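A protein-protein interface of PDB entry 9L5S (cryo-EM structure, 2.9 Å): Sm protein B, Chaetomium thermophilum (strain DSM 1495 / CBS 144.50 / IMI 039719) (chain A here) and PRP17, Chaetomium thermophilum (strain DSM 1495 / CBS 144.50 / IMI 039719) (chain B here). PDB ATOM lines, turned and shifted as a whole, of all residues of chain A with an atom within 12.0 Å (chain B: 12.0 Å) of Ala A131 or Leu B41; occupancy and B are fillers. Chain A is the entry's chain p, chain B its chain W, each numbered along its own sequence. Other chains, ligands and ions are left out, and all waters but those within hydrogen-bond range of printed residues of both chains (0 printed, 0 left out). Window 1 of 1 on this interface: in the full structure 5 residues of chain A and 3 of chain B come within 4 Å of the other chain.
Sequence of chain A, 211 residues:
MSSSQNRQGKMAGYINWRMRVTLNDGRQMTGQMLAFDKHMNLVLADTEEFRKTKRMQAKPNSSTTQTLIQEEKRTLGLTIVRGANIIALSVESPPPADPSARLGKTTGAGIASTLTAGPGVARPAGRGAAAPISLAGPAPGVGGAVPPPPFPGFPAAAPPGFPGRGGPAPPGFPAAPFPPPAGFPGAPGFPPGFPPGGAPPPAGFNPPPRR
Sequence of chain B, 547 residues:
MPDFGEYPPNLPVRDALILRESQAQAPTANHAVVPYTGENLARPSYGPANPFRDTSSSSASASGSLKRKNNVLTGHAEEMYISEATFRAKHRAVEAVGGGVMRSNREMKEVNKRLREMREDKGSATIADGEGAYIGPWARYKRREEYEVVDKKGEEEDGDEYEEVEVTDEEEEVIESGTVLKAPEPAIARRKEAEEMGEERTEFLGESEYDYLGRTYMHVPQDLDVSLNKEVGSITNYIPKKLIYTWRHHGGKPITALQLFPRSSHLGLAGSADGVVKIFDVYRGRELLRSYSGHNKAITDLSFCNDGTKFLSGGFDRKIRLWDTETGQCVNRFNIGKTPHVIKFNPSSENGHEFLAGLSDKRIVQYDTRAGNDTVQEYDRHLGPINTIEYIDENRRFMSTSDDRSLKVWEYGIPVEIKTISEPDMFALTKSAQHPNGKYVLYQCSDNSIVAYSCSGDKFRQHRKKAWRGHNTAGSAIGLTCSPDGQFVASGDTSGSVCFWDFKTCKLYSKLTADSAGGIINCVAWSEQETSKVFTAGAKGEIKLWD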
ATOM      1  N   GLY A 126     -10.217 -27.358  10.744  1.00  0.00           N
ATOM      2  CA  GLY A 126     -11.127 -26.235  10.683  1.00  0.00           C
ATOM      3  C   GLY A 126     -12.063 -26.218  11.872  1.00  0.00           C
ATOM      4  O   GLY A 126     -12.171 -27.214  12.592  1.00  0.00           O
ATOM      5  N   ARG A 127     -12.746 -25.097  12.094  1.00  0.00           N
ATOM      6  CA  ARG A 127     -13.693 -24.996  13.198  1.00  0.00           C
ATOM      7  C   ARG A 127     -15.040 -25.637  12.892  1.00  0.00           C
ATOM      8  O   ARG A 127     -15.975 -25.474  13.682  1.00  0.00           O
ATOM      9  CB  ARG A 127     -13.903 -23.531  13.582  1.00  0.00           C
ATOM     10  CG  ARG A 127     -12.724 -22.922  14.299  1.00  0.00           C
ATOM     11  CD  ARG A 127     -13.118 -21.742  15.166  1.00  0.00           C
ATOM     12  NE  ARG A 127     -11.948 -21.139  15.790  1.00  0.00           N
ATOM     13  CZ  ARG A 127     -11.461 -21.497  16.971  1.00  0.00           C
ATOM     14  NH1 ARG A 127     -12.036 -22.442  17.697  1.00  0.00           N
ATOM     15  NH2 ARG A 127     -10.368 -20.896  17.431  1.00  0.00           N
ATOM     16  N   GLY A 128     -15.165 -26.354  11.780  1.00  0.00           N
ATOM     17  CA  GLY A 128     -16.416 -26.989  11.430  1.00  0.00           C
ATOM     18  C   GLY A 128     -17.440 -25.990  10.936  1.00  0.00           C
ATOM     19  O   GLY A 128     -17.165 -24.809  10.713  1.00  0.00           O
ATOM     20  N   ALA A 129     -18.660 -26.488  10.762  1.00  0.00           N
ATOM     21  CA  ALA A 129     -19.785 -25.660  10.340  1.00  0.00           C
ATOM     22  C   ALA A 129     -20.478 -25.141  11.591  1.00  0.00           C
ATOM     23  O   ALA A 129     -21.150 -25.893  12.300  1.00  0.00           O
ATOM     24  CB  ALA A 129     -20.738 -26.454   9.455  1.00  0.00           C
ATOM     25  N   ALA A 130     -20.295 -23.851  11.873  1.00  0.00           N
ATOM     26  CA  ALA A 130     -20.975 -23.219  12.994  1.00  0.00           C
ATOM     27  C   ALA A 130     -22.481 -23.214  12.771  1.00  0.00           C
ATOM     28  O   ALA A 130     -22.956 -23.072  11.641  1.00  0.00           O
ATOM     29  CB  ALA A 130     -20.472 -21.789  13.184  1.00  0.00           C
ATOM     30  N   ALA A 131     -23.229 -23.381  13.853  1.00  0.00           N
ATOM     31  CA  ALA A 131     -24.683 -23.342  13.769  1.00  0.00           C
ATOM     32  C   ALA A 131     -25.130 -21.919  13.466  1.00  0.00           C
ATOM     33  O   ALA A 131     -24.841 -21.009  14.254  1.00  0.00           O
ATOM     34  CB  ALA A 131     -25.309 -23.835  15.070  1.00  0.00           C
ATOM     35  N   PRO A 132     -25.819 -21.677  12.350  1.00  0.00           N
ATOM     36  CA  PRO A 132     -26.195 -20.301  12.001  1.00  0.00           C
ATOM     37  C   PRO A 132     -27.318 -19.765  12.876  1.00  0.00           C
ATOM     38  O   PRO A 132     -28.485 -20.134  12.713  1.00  0.00           O
ATOM     39  CB  PRO A 132     -26.619 -20.415  10.530  1.00  0.00           C
ATOM     40  CG  PRO A 132     -27.019 -21.837  10.351  1.00  0.00           C
ATOM     41  CD  PRO A 132     -26.212 -22.652  11.317  1.00  0.00           C
ATOM     42  N   ILE A 133     -26.966 -18.886  13.808  1.00  0.00           N
ATOM     43  CA  ILE A 133     -27.931 -18.327  14.744  1.00  0.00           C
ATOM     44  C   ILE A 133     -28.480 -17.006  14.218  1.00  0.00           C
ATOM     45  O   ILE A 133     -28.779 -16.876  13.030  1.00  0.00           O
ATOM     46  CB  ILE A 133     -27.304 -18.143  16.138  1.00  0.00           C
ATOM     47  CG1 ILE A 133     -26.811 -19.486  16.682  1.00  0.00           C
ATOM     48  CG2 ILE A 133     -28.301 -17.503  17.092  1.00  0.00           C
ATOM     49  CD1 ILE A 133     -26.140 -19.393  18.034  1.00  0.00           C
ATOM     50  N   VAL B  34     -14.644 -14.434  10.789  1.00  0.00           N
ATOM     51  CA  VAL B  34     -15.605 -14.679   9.723  1.00  0.00           C
ATOM     52  C   VAL B  34     -15.474 -16.133   9.240  1.00  0.00           C
ATOM     53  O   VAL B  34     -14.366 -16.632   9.025  1.00  0.00           O
ATOM     54  CB  VAL B  34     -15.443 -13.616   8.580  1.00  0.00           C
ATOM     55  CG1 VAL B  34     -14.094 -13.714   7.884  1.00  0.00           C
ATOM     56  CG2 VAL B  34     -16.567 -13.719   7.559  1.00  0.00           C
ATOM     57  N   PRO B  35     -16.606 -16.851   9.146  1.00  0.00           N
ATOM     58  CA  PRO B  35     -17.976 -16.456   9.498  1.00  0.00           C
ATOM     59  C   PRO B  35     -18.337 -16.725  10.956  1.00  0.00           C
ATOM     60  O   PRO B  35     -19.481 -17.070  11.248  1.00  0.00           O
ATOM     61  CB  PRO B  35     -18.825 -17.320   8.571  1.00  0.00           C
ATOM     62  CG  PRO B  35     -18.026 -18.574   8.411  1.00  0.00           C
ATOM     63  CD  PRO B  35     -16.566 -18.222   8.604  1.00  0.00           C
ATOM     64  N   TYR B  36     -17.368 -16.575  11.855  1.00  0.00           N
ATOM     65  CA  TYR B  36     -17.562 -16.854  13.269  1.00  0.00           C
ATOM     66  C   TYR B  36     -17.716 -15.595  14.113  1.00  0.00           C
ATOM     67  O   TYR B  36     -17.893 -15.700  15.330  1.00  0.00           O
ATOM     68  CB  TYR B  36     -16.394 -17.692  13.795  1.00  0.00           C
ATOM     69  CG  TYR B  36     -16.190 -18.979  13.029  1.00  0.00           C
ATOM     70  CD1 TYR B  36     -17.222 -19.895  12.885  1.00  0.00           C
ATOM     71  CD2 TYR B  36     -14.966 -19.270  12.438  1.00  0.00           C
ATOM     72  CE1 TYR B  36     -17.041 -21.071  12.183  1.00  0.00           C
ATOM     73  CE2 TYR B  36     -14.775 -20.443  11.733  1.00  0.00           C
ATOM     74  CZ  TYR B  36     -15.817 -21.338  11.608  1.00  0.00           C
ATOM     75  OH  TYR B  36     -15.632 -22.508  10.908  1.00  0.00           O
ATOM     76  N   THR B  37     -17.650 -14.414  13.502  1.00  0.00           N
ATOM     77  CA  THR B  37     -17.771 -13.172  14.250  1.00  0.00           C
ATOM     78  C   THR B  37     -19.214 -12.929  14.680  1.00  0.00           C
ATOM     79  O   THR B  37     -20.150 -13.595  14.230  1.00  0.00           O
ATOM     80  CB  THR B  37     -17.275 -11.987  13.424  1.00  0.00           C
ATOM     81  OG1 THR B  37     -18.119 -11.813  12.281  1.00  0.00           O
ATOM     82  CG2 THR B  37     -15.843 -12.205  12.975  1.00  0.00           C
ATOM     83  N   GLY B  38     -19.382 -11.951  15.572  1.00  0.00           N
ATOM     84  CA  GLY B  38     -20.691 -11.684  16.144  1.00  0.00           C
ATOM     85  C   GLY B  38     -21.699 -11.122  15.164  1.00  0.00           C
ATOM     86  O   GLY B  38     -22.883 -11.460  15.233  1.00  0.00           O
ATOM     87  N   GLU B  39     -21.258 -10.255  14.250  1.00  0.00           N
ATOM     88  CA  GLU B  39     -22.197  -9.672  13.295  1.00  0.00           C
ATOM     89  C   GLU B  39     -22.636 -10.687  12.246  1.00  0.00           C
ATOM     90  O   GLU B  39     -23.711 -10.535  11.654  1.00  0.00           O
ATOM     91  CB  GLU B  39     -21.589  -8.430  12.635  1.00  0.00           C
ATOM     92  CG  GLU B  39     -20.596  -8.694  11.509  1.00  0.00           C
ATOM     93  CD  GLU B  39     -19.169  -8.867  12.002  1.00  0.00           C
ATOM     94  OE1 GLU B  39     -18.972  -9.130  13.207  1.00  0.00           O
ATOM     95  OE2 GLU B  39     -18.240  -8.742  11.177  1.00  0.00           O
ATOM     96  N   ASN B  40     -21.828 -11.722  12.001  1.00  0.00           N
ATOM     97  CA  ASN B  40     -22.235 -12.777  11.079  1.00  0.00           C
ATOM     98  C   ASN B  40     -23.243 -13.723  11.721  1.00  0.00           C
ATOM     99  O   ASN B  40     -24.187 -14.167  11.059  1.00  0.00           O
ATOM    100  CB  ASN B  40     -21.006 -13.547  10.596  1.00  0.00           C
ATOM    101  CG  ASN B  40     -20.066 -12.686   9.780  1.00  0.00           C
ATOM    102  OD1 ASN B  40     -18.856 -12.900   9.780  1.00  0.00           O
ATOM    103  ND2 ASN B  40     -20.620 -11.706   9.078  1.00  0.00           N
ATOM    104  N   LEU B  41     -23.056 -14.051  13.000  1.00  0.00           N
ATOM    105  CA  LEU B  41     -24.037 -14.869  13.705  1.00  0.00           C
ATOM    106  C   LEU B  41     -25.291 -14.084  14.064  1.00  0.00           C
ATOM    107  O   LEU B  41     -26.344 -14.692  14.286  1.00  0.00           O
ATOM    108  CB  LEU B  41     -23.427 -15.476  14.975  1.00  0.00           C
ATOM    109  CG  LEU B  41     -22.594 -16.766  14.917  1.00  0.00           C
ATOM    110  CD1 LEU B  41     -23.462 -17.929  14.451  1.00  0.00           C
ATOM    111  CD2 LEU B  41     -21.334 -16.657  14.065  1.00  0.00           C
ATOM    112  N   ALA B  42     -25.205 -12.757  14.127  1.00  0.00           N
ATOM    113  CA  ALA B  42     -26.342 -11.925  14.495  1.00  0.00           C
ATOM    114  C   ALA B  42     -27.352 -11.763  13.369  1.00  0.00           C
ATOM    115  O   ALA B  42     -28.547 -11.598  13.644  1.00  0.00           O
ATOM    116  CB  ALA B  42     -25.859 -10.544  14.947  1.00  0.00           C
ATOM    117  N   ARG B  43     -26.907 -11.789  12.118  1.00  0.00           N
ATOM    118  CA  ARG B  43     -27.825 -11.599  11.002  1.00  0.00           C
ATOM    119  C   ARG B  43     -28.715 -12.829  10.842  1.00  0.00           C
ATOM    120  O   ARG B  43     -28.244 -13.961  11.009  1.00  0.00           O
ATOM    121  CB  ARG B  43     -27.050 -11.293   9.712  1.00  0.00           C
ATOM    122  CG  ARG B  43     -26.202 -12.429   9.154  1.00  0.00           C
ATOM    123  CD  ARG B  43     -25.467 -12.027   7.884  1.00  0.00           C
ATOM    124  NE  ARG B  43     -24.481 -10.979   8.120  1.00  0.00           N
ATOM    125  CZ  ARG B  43     -24.610  -9.722   7.720  1.00  0.00           C
ATOM    126  NH1 ARG B  43     -25.683  -9.313   7.062  1.00  0.00           N
ATOM    127  NH2 ARG B  43     -23.639  -8.853   7.984  1.00  0.00           N
ATOM    128  N   PRO B  44     -30.012 -12.653  10.592  1.00  0.00           N
ATOM    129  CA  PRO B  44     -30.895 -13.812  10.431  1.00  0.00           C
ATOM    130  C   PRO B  44     -30.988 -14.273   8.987  1.00  0.00           C
ATOM    131  O   PRO B  44     -30.367 -13.683   8.097  1.00  0.00           O
ATOM    132  CB  PRO B  44     -32.242 -13.290  10.938  1.00  0.00           C
ATOM    133  CG  PRO B  44     -32.209 -11.831  10.598  1.00  0.00           C
ATOM    134  CD  PRO B  44     -30.763 -11.385  10.634  1.00  0.00           C
ATOM    135  N   SER B  45     -31.772 -15.318   8.742  1.00  0.00           N
ATOM    136  CA  SER B  45     -32.031 -15.798   7.391  1.00  0.00           C
ATOM    137  C   SER B  45     -33.247 -15.065   6.840  1.00  0.00           C
ATOM    138  O   SER B  45     -34.302 -15.030   7.484  1.00  0.00           O
ATOM    139  CB  SER B  45     -32.256 -17.309   7.384  1.00  0.00           C
ATOM    140  OG  SER B  45     -33.479 -17.643   8.016  1.00  0.00           O
ATOM    141  N   TYR B  46     -33.101 -14.481   5.654  1.00  0.00           N
ATOM    142  CA  TYR B  46     -34.168 -13.681   5.076  1.00  0.00           C
ATOM    143  C   TYR B  46     -35.288 -14.570   4.546  1.00  0.00           C
ATOM    144  O   TYR B  46     -35.193 -15.800   4.525  1.00  0.00           O
ATOM    145  CB  TYR B  46     -33.637 -12.811   3.939  1.00  0.00           C
ATOM    146  CG  TYR B  46     -32.938 -11.552   4.385  1.00  0.00           C
ATOM    147  CD1 TYR B  46     -33.550 -10.667   5.259  1.00  0.00           C
ATOM    148  CD2 TYR B  46     -31.665 -11.244   3.921  1.00  0.00           C
ATOM    149  CE1 TYR B  46     -32.910  -9.515   5.668  1.00  0.00           C
ATOM    150  CE2 TYR B  46     -31.018 -10.092   4.321  1.00  0.00           C
ATOM    151  CZ  TYR B  46     -31.646  -9.230   5.194  1.00  0.00           C
ATOM    152  OH  TYR B  46     -31.007  -8.080   5.597  1.00  0.00           O
ATOM    153  N   LYS B  69     -30.734 -30.867   9.315  1.00  0.00           N
ATOM    154  CA  LYS B  69     -31.797 -31.335  10.198  1.00  0.00           C
ATOM    155  C   LYS B  69     -31.345 -32.546  11.034  1.00  0.00           C
ATOM    156  O   LYS B  69     -30.161 -32.658  11.357  1.00  0.00           O
ATOM    157  CB  LYS B  69     -33.069 -31.623   9.373  1.00  0.00           C
ATOM    158  CG  LYS B  69     -33.017 -32.796   8.385  1.00  0.00           C
ATOM    159  CD  LYS B  69     -34.337 -32.935   7.641  1.00  0.00           C
ATOM    160  CE  LYS B  69     -34.288 -34.069   6.632  1.00  0.00           C
ATOM    161  NZ  LYS B  69     -34.170 -35.390   7.308  1.00  0.00           N
ATOM    162  N   HIS B  76     -31.817 -36.091  16.435  1.00  0.00           N
ATOM    163  CA  HIS B  76     -30.478 -35.602  16.143  1.00  0.00           C
ATOM    164  C   HIS B  76     -29.517 -36.119  17.201  1.00  0.00           C
ATOM    165  O   HIS B  76     -29.724 -35.892  18.398  1.00  0.00           O
ATOM    166  CB  HIS B  76     -30.444 -34.074  16.094  1.00  0.00           C
ATOM    167  CG  HIS B  76     -29.083 -33.513  15.827  1.00  0.00           C
ATOM    168  ND1 HIS B  76     -28.366 -33.813  14.689  1.00  0.00           N
ATOM    169  CD2 HIS B  76     -28.308 -32.668  16.548  1.00  0.00           C
ATOM    170  CE1 HIS B  76     -27.208 -33.180  14.720  1.00  0.00           C
ATOM    171  NE2 HIS B  76     -27.147 -32.478  15.838  1.00  0.00           N
ATOM    172  N   GLU B  78     -25.328 -36.416  18.165  1.00  0.00           N
ATOM    173  CA  GLU B  78     -23.961 -35.988  17.912  1.00  0.00           C
ATOM    174  C   GLU B  78     -23.029 -36.644  18.919  1.00  0.00           C
ATOM    175  O   GLU B  78     -23.439 -37.004  20.026  1.00  0.00           O
ATOM    176  CB  GLU B  78     -23.823 -34.459  17.990  1.00  0.00           C
ATOM    177  CG  GLU B  78     -24.075 -33.878  19.372  1.00  0.00           C
ATOM    178  CD  GLU B  78     -23.993 -32.365  19.396  1.00  0.00           C
ATOM    179  OE1 GLU B  78     -23.762 -31.763  18.327  1.00  0.00           O
ATOM    180  OE2 GLU B  78     -24.153 -31.777  20.486  1.00  0.00           O
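Printed residues of chain A that touch a printed residue of chain B: Arg A127, Gly A128, Ala A130, Ala A131 and Ile A133. Hydrophobic or aromatic side chains of chain A within 4 Å of the printed part of chain B: Ala A130. Of the 16 printed residues of chain B, 3 touch a printed residue of chain A. Printed residues of chain B that touch a printed residue of chain A: Tyr B36, Leu B41 and Arg B43. Among the printed residues, 6 pairs touch across the chains.
Of the printed residues of chain B, Arg A127 touches Tyr B36 (3.3 Å). Printed residues of chain B within 4 Å of Gly A128: Tyr B36 (2.8 Å). No residue of chain B comes within 4 Å of Ala A129. Of chain B, only Tyr B36 (3.6 Å) comes within 4 Å of Ala A130. Of chain B, only Leu B41 (3.4 Å) comes within 4 Å of Ala A131. No residue of chain B comes within 4 Å of Pro A132. Printed residues of chain A within 4 Å of Tyr B36: Arg A127 (3.3 Å), Gly A128 (2.8 Å) and Ala A130 (3.6 Å). No residue of chain A comes within 4 Å of Gly B38. Glu B39 touches none of the printed residues of chain A. No residue of chain A comes within 4 Å of Asn B40. Of chain A, only Ala A131 and Ile A133 come within 4 Å of Leu B41. No residue of chain A comes within 4 Å of Ala B42. Printed residues of chain A within 4 Å of Arg B43: Ile A133. The nearest residue of chain B that does not touch Ala A131 is Tyr B36 (6.8 Å). The nearest printed residue of chain A that does not touch Tyr B36 is Ala A129 (5.0 Å).
Tyr B36 touches Arg A127 (OH to CB, 3.3 Å). Ala A130 touches Tyr B36. CD1 of Leu B41 touches O of Ala A131 (3.4 Å). C of Ile A133 touches O of Leu B41 (3.1 Å). Arg B43 touches Ile A133.
The side-chain hydroxyl (OH) of Tyr B36 sits at hydrogen-bond distance from the backbone carbonyl oxygen (O) of Gly A128 (2.8 Å).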
